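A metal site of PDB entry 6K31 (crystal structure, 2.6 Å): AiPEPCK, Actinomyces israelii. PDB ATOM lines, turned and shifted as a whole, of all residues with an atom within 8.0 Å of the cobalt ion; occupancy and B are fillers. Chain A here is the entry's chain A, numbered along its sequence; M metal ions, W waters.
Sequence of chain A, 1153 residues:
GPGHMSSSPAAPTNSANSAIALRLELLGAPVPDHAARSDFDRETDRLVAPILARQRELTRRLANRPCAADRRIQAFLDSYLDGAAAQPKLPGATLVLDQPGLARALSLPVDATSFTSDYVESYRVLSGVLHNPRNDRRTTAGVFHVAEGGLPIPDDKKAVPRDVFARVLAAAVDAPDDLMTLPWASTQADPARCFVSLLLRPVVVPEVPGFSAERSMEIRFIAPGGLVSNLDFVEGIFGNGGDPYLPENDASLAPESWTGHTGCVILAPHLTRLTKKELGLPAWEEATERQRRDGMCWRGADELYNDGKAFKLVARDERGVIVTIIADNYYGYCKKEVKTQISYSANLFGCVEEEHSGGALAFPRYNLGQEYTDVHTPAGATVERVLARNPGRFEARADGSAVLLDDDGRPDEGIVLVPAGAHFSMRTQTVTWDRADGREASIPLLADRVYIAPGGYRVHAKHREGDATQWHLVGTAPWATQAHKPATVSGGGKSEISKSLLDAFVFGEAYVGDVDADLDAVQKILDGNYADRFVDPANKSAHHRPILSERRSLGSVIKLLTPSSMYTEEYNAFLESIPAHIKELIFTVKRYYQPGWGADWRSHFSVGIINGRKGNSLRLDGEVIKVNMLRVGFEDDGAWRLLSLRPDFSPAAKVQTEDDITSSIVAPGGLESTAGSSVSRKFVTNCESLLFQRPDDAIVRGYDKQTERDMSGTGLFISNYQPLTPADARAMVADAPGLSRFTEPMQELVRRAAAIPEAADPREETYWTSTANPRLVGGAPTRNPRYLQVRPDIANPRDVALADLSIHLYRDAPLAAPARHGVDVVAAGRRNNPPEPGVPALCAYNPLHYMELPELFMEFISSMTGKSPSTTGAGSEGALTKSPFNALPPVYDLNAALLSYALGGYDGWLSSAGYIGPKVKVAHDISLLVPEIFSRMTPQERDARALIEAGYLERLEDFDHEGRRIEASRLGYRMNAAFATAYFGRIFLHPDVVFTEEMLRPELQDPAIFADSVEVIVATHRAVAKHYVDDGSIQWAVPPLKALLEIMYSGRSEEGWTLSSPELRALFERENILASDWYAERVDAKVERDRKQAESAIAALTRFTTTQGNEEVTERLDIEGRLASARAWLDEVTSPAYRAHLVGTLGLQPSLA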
ATOM      1  N   ARG A 138      -3.636   2.923   4.776  1.00  0.00           N
ATOM      2  CA  ARG A 138      -3.397   3.622   6.038  1.00  0.00           C
ATOM      3  C   ARG A 138      -2.485   2.785   6.920  1.00  0.00           C
ATOM      4  O   ARG A 138      -2.477   1.582   6.845  1.00  0.00           O
ATOM      5  CB  ARG A 138      -4.732   3.822   6.760  1.00  0.00           C
ATOM      6  CG  ARG A 138      -4.731   4.897   7.841  1.00  0.00           C
ATOM      7  CD  ARG A 138      -6.134   5.463   8.081  1.00  0.00           C
ATOM      8  NE  ARG A 138      -7.068   4.397   8.387  1.00  0.00           N
ATOM      9  CZ  ARG A 138      -7.117   3.734   9.546  1.00  0.00           C
ATOM     10  NH1 ARG A 138      -6.298   4.023  10.548  1.00  0.00           N
ATOM     11  NH2 ARG A 138      -7.996   2.764   9.699  1.00  0.00           N
ATOM     12  N   LYS A 335     -10.985  11.028   6.509  1.00  0.00           N
ATOM     13  CA  LYS A 335     -12.116  10.463   7.170  1.00  0.00           C
ATOM     14  C   LYS A 335     -11.836  10.277   8.689  1.00  0.00           C
ATOM     15  O   LYS A 335     -12.668  10.594   9.544  1.00  0.00           O
ATOM     16  CB  LYS A 335     -12.381   9.087   6.498  1.00  0.00           C
ATOM     17  CG  LYS A 335     -13.622   8.381   6.942  1.00  0.00           C
ATOM     18  CD  LYS A 335     -13.664   6.914   6.541  1.00  0.00           C
ATOM     19  CE  LYS A 335     -14.360   6.111   7.643  1.00  0.00           C
ATOM     20  NZ  LYS A 335     -15.328   5.116   7.149  1.00  0.00           N
ATOM     21  N   LYS A 336     -10.680   9.734   9.028  1.00  0.00           N
ATOM     22  CA  LYS A 336     -10.407   9.389  10.429  1.00  0.00           C
ATOM     23  C   LYS A 336      -9.959  10.602  11.191  1.00  0.00           C
ATOM     24  O   LYS A 336     -10.003  10.598  12.430  1.00  0.00           O
ATOM     25  CB  LYS A 336      -9.430   8.218  10.592  1.00  0.00           C
ATOM     26  CG  LYS A 336      -9.970   6.868  10.077  1.00  0.00           C
ATOM     27  CD  LYS A 336     -11.182   6.330  10.875  1.00  0.00           C
ATOM     28  CE  LYS A 336     -11.569   4.874  10.540  1.00  0.00           C
ATOM     29  NZ  LYS A 336     -12.633   4.269  11.426  1.00  0.00           N
ATOM     30  N   LYS A 339     -13.261  12.076  12.320  1.00  0.00           N
ATOM     31  CA  LYS A 339     -13.568  11.252  13.465  1.00  0.00           C
ATOM     32  C   LYS A 339     -12.892  11.723  14.739  1.00  0.00           C
ATOM     33  O   LYS A 339     -13.559  11.980  15.736  1.00  0.00           O
ATOM     34  CB  LYS A 339     -13.182   9.787  13.220  1.00  0.00           C
ATOM     35  CG  LYS A 339     -13.728   8.842  14.271  1.00  0.00           C
ATOM     36  CD  LYS A 339     -13.307   7.419  13.958  1.00  0.00           C
ATOM     37  CE  LYS A 339     -13.726   6.508  15.103  1.00  0.00           C
ATOM     38  NZ  LYS A 339     -15.211   6.258  15.121  1.00  0.00           N
ATOM     39  N   HIS A 356     -16.785   4.192  17.706  1.00  0.00           N
ATOM     40  CA  HIS A 356     -16.442   3.412  16.509  1.00  0.00           C
ATOM     41  C   HIS A 356     -17.370   2.195  16.537  1.00  0.00           C
ATOM     42  O   HIS A 356     -17.118   1.269  17.275  1.00  0.00           O
ATOM     43  CB  HIS A 356     -14.936   3.059  16.612  1.00  0.00           C
ATOM     44  CG  HIS A 356     -14.313   2.563  15.333  1.00  0.00           C
ATOM     45  ND1 HIS A 356     -13.100   1.927  15.306  1.00  0.00           N
ATOM     46  CD2 HIS A 356     -14.705   2.653  14.050  1.00  0.00           C
ATOM     47  CE1 HIS A 356     -12.762   1.662  14.066  1.00  0.00           C
ATOM     48  NE2 HIS A 356     -13.697   2.137  13.271  1.00  0.00           N
ATOM     49  N   SER A 357     -18.484   2.224  15.821  1.00  0.00           N
ATOM     50  CA  SER A 357     -19.561   1.217  16.056  1.00  0.00           C
ATOM     51  C   SER A 357     -20.550   1.088  14.938  1.00  0.00           C
ATOM     52  O   SER A 357     -20.791   2.049  14.190  1.00  0.00           O
ATOM     53  CB  SER A 357     -20.365   1.542  17.305  1.00  0.00           C
ATOM     54  OG  SER A 357     -21.129   2.682  17.058  1.00  0.00           O
ATOM     55  N   THR A 488     -15.295  -2.816  18.802  1.00  0.00           N
ATOM     56  CA  THR A 488     -15.191  -4.154  18.228  1.00  0.00           C
ATOM     57  C   THR A 488     -14.009  -4.137  17.297  1.00  0.00           C
ATOM     58  O   THR A 488     -13.995  -3.407  16.314  1.00  0.00           O
ATOM     59  CB  THR A 488     -16.450  -4.455  17.398  1.00  0.00           C
ATOM     60  OG1 THR A 488     -17.578  -4.541  18.283  1.00  0.00           O
ATOM     61  CG2 THR A 488     -16.281  -5.710  16.641  1.00  0.00           C
ATOM     62  N   SER A 490     -11.008  -5.025  14.647  1.00  0.00           N
ATOM     63  CA  SER A 490     -11.067  -5.416  13.241  1.00  0.00           C
ATOM     64  C   SER A 490     -11.091  -6.928  13.212  1.00  0.00           C
ATOM     65  O   SER A 490     -10.398  -7.575  13.983  1.00  0.00           O
ATOM     66  CB  SER A 490      -9.808  -4.881  12.564  1.00  0.00           C
ATOM     67  OG  SER A 490      -9.623  -5.424  11.271  1.00  0.00           O
ATOM     68  N   LYS A 494     -18.026  -5.580  13.098  1.00  0.00           N
ATOM     69  CA  LYS A 494     -18.808  -4.347  13.411  1.00  0.00           C
ATOM     70  C   LYS A 494     -19.889  -4.044  12.360  1.00  0.00           C
ATOM     71  O   LYS A 494     -21.048  -3.797  12.691  1.00  0.00           O
ATOM     72  CB  LYS A 494     -17.859  -3.185  13.534  1.00  0.00           C
ATOM     73  CG  LYS A 494     -18.446  -1.811  13.324  1.00  0.00           C
ATOM     74  CD  LYS A 494     -17.484  -0.720  13.774  1.00  0.00           C
ATOM     75  CE  LYS A 494     -16.231  -0.591  12.909  1.00  0.00           C
ATOM     76  NZ  LYS A 494     -16.483   0.261  11.682  1.00  0.00           N
ATOM     77  N   SER A 495     -19.511  -4.147  11.105  1.00  0.00           N
ATOM     78  CA  SER A 495     -20.462  -3.961  10.031  1.00  0.00           C
ATOM     79  C   SER A 495     -21.438  -5.083   9.878  1.00  0.00           C
ATOM     80  O   SER A 495     -22.521  -4.874   9.352  1.00  0.00           O
ATOM     81  CB  SER A 495     -19.746  -3.752   8.704  1.00  0.00           C
ATOM     82  OG  SER A 495     -19.115  -2.490   8.824  1.00  0.00           O
ATOM     83  N   ASP A 659     -22.423   2.880  11.376  1.00  0.00           N
ATOM     84  CA  ASP A 659     -21.417   2.034  10.704  1.00  0.00           C
ATOM     85  C   ASP A 659     -20.017   2.209  11.209  1.00  0.00           C
ATOM     86  O   ASP A 659     -19.375   1.197  11.503  1.00  0.00           O
ATOM     87  CB  ASP A 659     -21.380   2.180   9.204  1.00  0.00           C
ATOM     88  CG  ASP A 659     -20.548   1.054   8.552  1.00  0.00           C
ATOM     89  OD1 ASP A 659     -20.857  -0.158   8.845  1.00  0.00           O
ATOM     90  OD2 ASP A 659     -19.567   1.366   7.779  1.00  0.00           O
ATOM     91  N   ASP A 660     -19.521   3.445  11.274  1.00  0.00           N
ATOM     92  CA  ASP A 660     -18.107   3.627  11.619  1.00  0.00           C
ATOM     93  C   ASP A 660     -17.891   4.824  12.482  1.00  0.00           C
ATOM     94  O   ASP A 660     -17.124   4.768  13.439  1.00  0.00           O
ATOM     95  CB  ASP A 660     -17.219   3.573  10.337  1.00  0.00           C
ATOM     96  CG  ASP A 660     -15.723   3.697  10.621  1.00  0.00           C
ATOM     97  OD1 ASP A 660     -15.052   2.761  11.091  1.00  0.00           O
ATOM     98  OD2 ASP A 660     -15.190   4.788  10.403  1.00  0.00           O
ATOM     99  N   ILE A 661     -18.501   5.930  12.131  1.00  0.00           N
ATOM    100  CA  ILE A 661     -18.337   7.109  12.932  1.00  0.00           C
ATOM    101  C   ILE A 661     -19.717   7.387  13.487  1.00  0.00           C
ATOM    102  O   ILE A 661     -20.665   7.626  12.710  1.00  0.00           O
ATOM    103  CB  ILE A 661     -17.807   8.273  12.079  1.00  0.00           C
ATOM    104  CG1 ILE A 661     -16.403   7.947  11.575  1.00  0.00           C
ATOM    105  CG2 ILE A 661     -17.718   9.603  12.869  1.00  0.00           C
ATOM    106  CD1 ILE A 661     -15.961   8.849  10.441  1.00  0.00           C
ATOM    107  N   GLU A 688     -21.703   9.934   9.000  1.00  0.00           N
ATOM    108  CA  GLU A 688     -21.363   9.851   7.583  1.00  0.00           C
ATOM    109  C   GLU A 688     -22.574   9.599   6.661  1.00  0.00           C
ATOM    110  O   GLU A 688     -23.379   8.741   6.959  1.00  0.00           O
ATOM    111  CB  GLU A 688     -20.399   8.684   7.365  1.00  0.00           C
ATOM    112  CG  GLU A 688     -19.128   8.683   8.175  1.00  0.00           C
ATOM    113  CD  GLU A 688     -18.208   7.494   7.822  1.00  0.00           C
ATOM    114  OE1 GLU A 688     -18.563   6.308   8.128  1.00  0.00           O
ATOM    115  OE2 GLU A 688     -17.113   7.729   7.233  1.00  0.00           O
ATOM    116  N   PHE A 692     -17.018   4.339   3.509  1.00  0.00           N
ATOM    117  CA  PHE A 692     -15.814   3.956   2.817  1.00  0.00           C
ATOM    118  C   PHE A 692     -15.572   2.414   2.940  1.00  0.00           C
ATOM    119  O   PHE A 692     -14.921   1.955   3.866  1.00  0.00           O
ATOM    120  CB  PHE A 692     -14.667   4.816   3.415  1.00  0.00           C
ATOM    121  CG  PHE A 692     -13.440   4.894   2.579  1.00  0.00           C
ATOM    122  CD1 PHE A 692     -13.504   5.189   1.222  1.00  0.00           C
ATOM    123  CD2 PHE A 692     -12.206   4.748   3.173  1.00  0.00           C
ATOM    124  CE1 PHE A 692     -12.350   5.275   0.456  1.00  0.00           C
ATOM    125  CE2 PHE A 692     -11.050   4.843   2.410  1.00  0.00           C
ATOM    126  CZ  PHE A 692     -11.128   5.098   1.050  1.00  0.00           C
ATOM    127  N   ARG A 786     -11.247   0.193  -2.573  1.00  0.00           N
ATOM    128  CA  ARG A 786     -12.187   1.061  -1.829  1.00  0.00           C
ATOM    129  C   ARG A 786     -13.202   1.761  -2.702  1.00  0.00           C
ATOM    130  O   ARG A 786     -12.924   2.097  -3.850  1.00  0.00           O
ATOM    131  CB  ARG A 786     -11.432   2.144  -1.065  1.00  0.00           C
ATOM    132  CG  ARG A 786     -10.556   1.657   0.082  1.00  0.00           C
ATOM    133  CD  ARG A 786     -11.340   1.436   1.366  1.00  0.00           C
ATOM    134  NE  ARG A 786     -10.472   1.050   2.460  1.00  0.00           N
ATOM    135  CZ  ARG A 786     -10.788   1.065   3.736  1.00  0.00           C
ATOM    136  NH1 ARG A 786     -11.975   1.499   4.163  1.00  0.00           N
ATOM    137  NH2 ARG A 786      -9.872   0.681   4.613  1.00  0.00           N
ATOM    138  N   GLU A 877      -6.039  -2.458  20.132  1.00  0.00           N
ATOM    139  CA  GLU A 877      -6.507  -1.238  19.432  1.00  0.00           C
ATOM    140  C   GLU A 877      -6.829  -0.070  20.395  1.00  0.00           C
ATOM    141  O   GLU A 877      -7.457   0.886  19.991  1.00  0.00           O
ATOM    142  CB  GLU A 877      -7.748  -1.528  18.591  1.00  0.00           C
ATOM    143  CG  GLU A 877      -7.461  -2.450  17.422  1.00  0.00           C
ATOM    144  CD  GLU A 877      -8.621  -2.597  16.432  1.00  0.00           C
ATOM    145  OE1 GLU A 877      -9.616  -1.845  16.522  1.00  0.00           O
ATOM    146  OE2 GLU A 877      -8.541  -3.464  15.528  1.00  0.00           O
ATOM    147  N   THR A 881     -11.347   0.761  20.888  1.00  0.00           N
ATOM    148  CA  THR A 881     -10.853   0.631  19.508  1.00  0.00           C
ATOM    149  C   THR A 881     -10.520   1.947  18.894  1.00  0.00           C
ATOM    150  O   THR A 881     -10.422   2.007  17.678  1.00  0.00           O
ATOM    151  CB  THR A 881     -11.805  -0.138  18.535  1.00  0.00           C
ATOM    152  OG1 THR A 881     -12.956   0.633  18.120  1.00  0.00           O
ATOM    153  CG2 THR A 881     -12.237  -1.496  19.112  1.00  0.00           C
ATOM    154  N   PHE A 885      -7.638   7.292  16.776  1.00  0.00           N
ATOM    155  CA  PHE A 885      -8.583   8.324  16.482  1.00  0.00           C
ATOM    156  C   PHE A 885      -8.974   9.104  17.727  1.00  0.00           C
ATOM    157  O   PHE A 885     -10.083   9.567  17.828  1.00  0.00           O
ATOM    158  CB  PHE A 885      -9.868   7.702  15.988  1.00  0.00           C
ATOM    159  CG  PHE A 885      -9.677   6.525  15.113  1.00  0.00           C
ATOM    160  CD1 PHE A 885      -8.914   6.630  13.963  1.00  0.00           C
ATOM    161  CD2 PHE A 885     -10.322   5.329  15.403  1.00  0.00           C
ATOM    162  CE1 PHE A 885      -8.787   5.538  13.099  1.00  0.00           C
ATOM    163  CE2 PHE A 885     -10.178   4.237  14.558  1.00  0.00           C
ATOM    164  CZ  PHE A 885      -9.431   4.342  13.389  1.00  0.00           C
HETATM  165 CO    CO M   1     -13.115   2.176  11.218  1.00  0.00          CO
HETATM  166  O   HOH W   1     -10.886   1.814  11.620  1.00  0.00           O
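The side-chain amino group (NZ) of Lys 494 is in hydrogen-bond range of the backbone carbonyl oxygen (O) of Asp 659, 3.0 Å away.
The side-chain carboxylate (OD1) of Asp 660 lies close to the side-chain amino group (NZ) of Lys 494 (2.9 Å).
The side-chain carboxylate (OD2) of Asp 660 is in salt-bridge range of the side-chain amino group (NZ) of Lys 335 (3.3 Å).
N of Asp 660 is in hydrogen-bond range of O of Ser 357, 3.5 Å away.
A ring nitrogen (ND1) of His 356 lies within hydrogen-bond range of the side-chain hydroxyl (OG1) of Thr 881.
The side-chain amino group (NZ) of Lys 339 is in hydrogen-bond range of the backbone carbonyl oxygen (O) of Asp 660, at 3.0 Å.
Lys 494 touches the cobalt ion (NZ to CO, 3.9 Å).
Of the 19 residues printed, 4 come within 4 Å of the cobalt ion.
The nearest printed residue that does not touch the cobalt ion is Phe 885 (4.8 Å).
The cobalt ion is bound by the side-chain carboxylate of Asp 660, a ring nitrogen (NE2) of His 356, the side-chain amino group of Lys 336 and water W1.
The cobalt ion has four donor atoms within binding distance.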
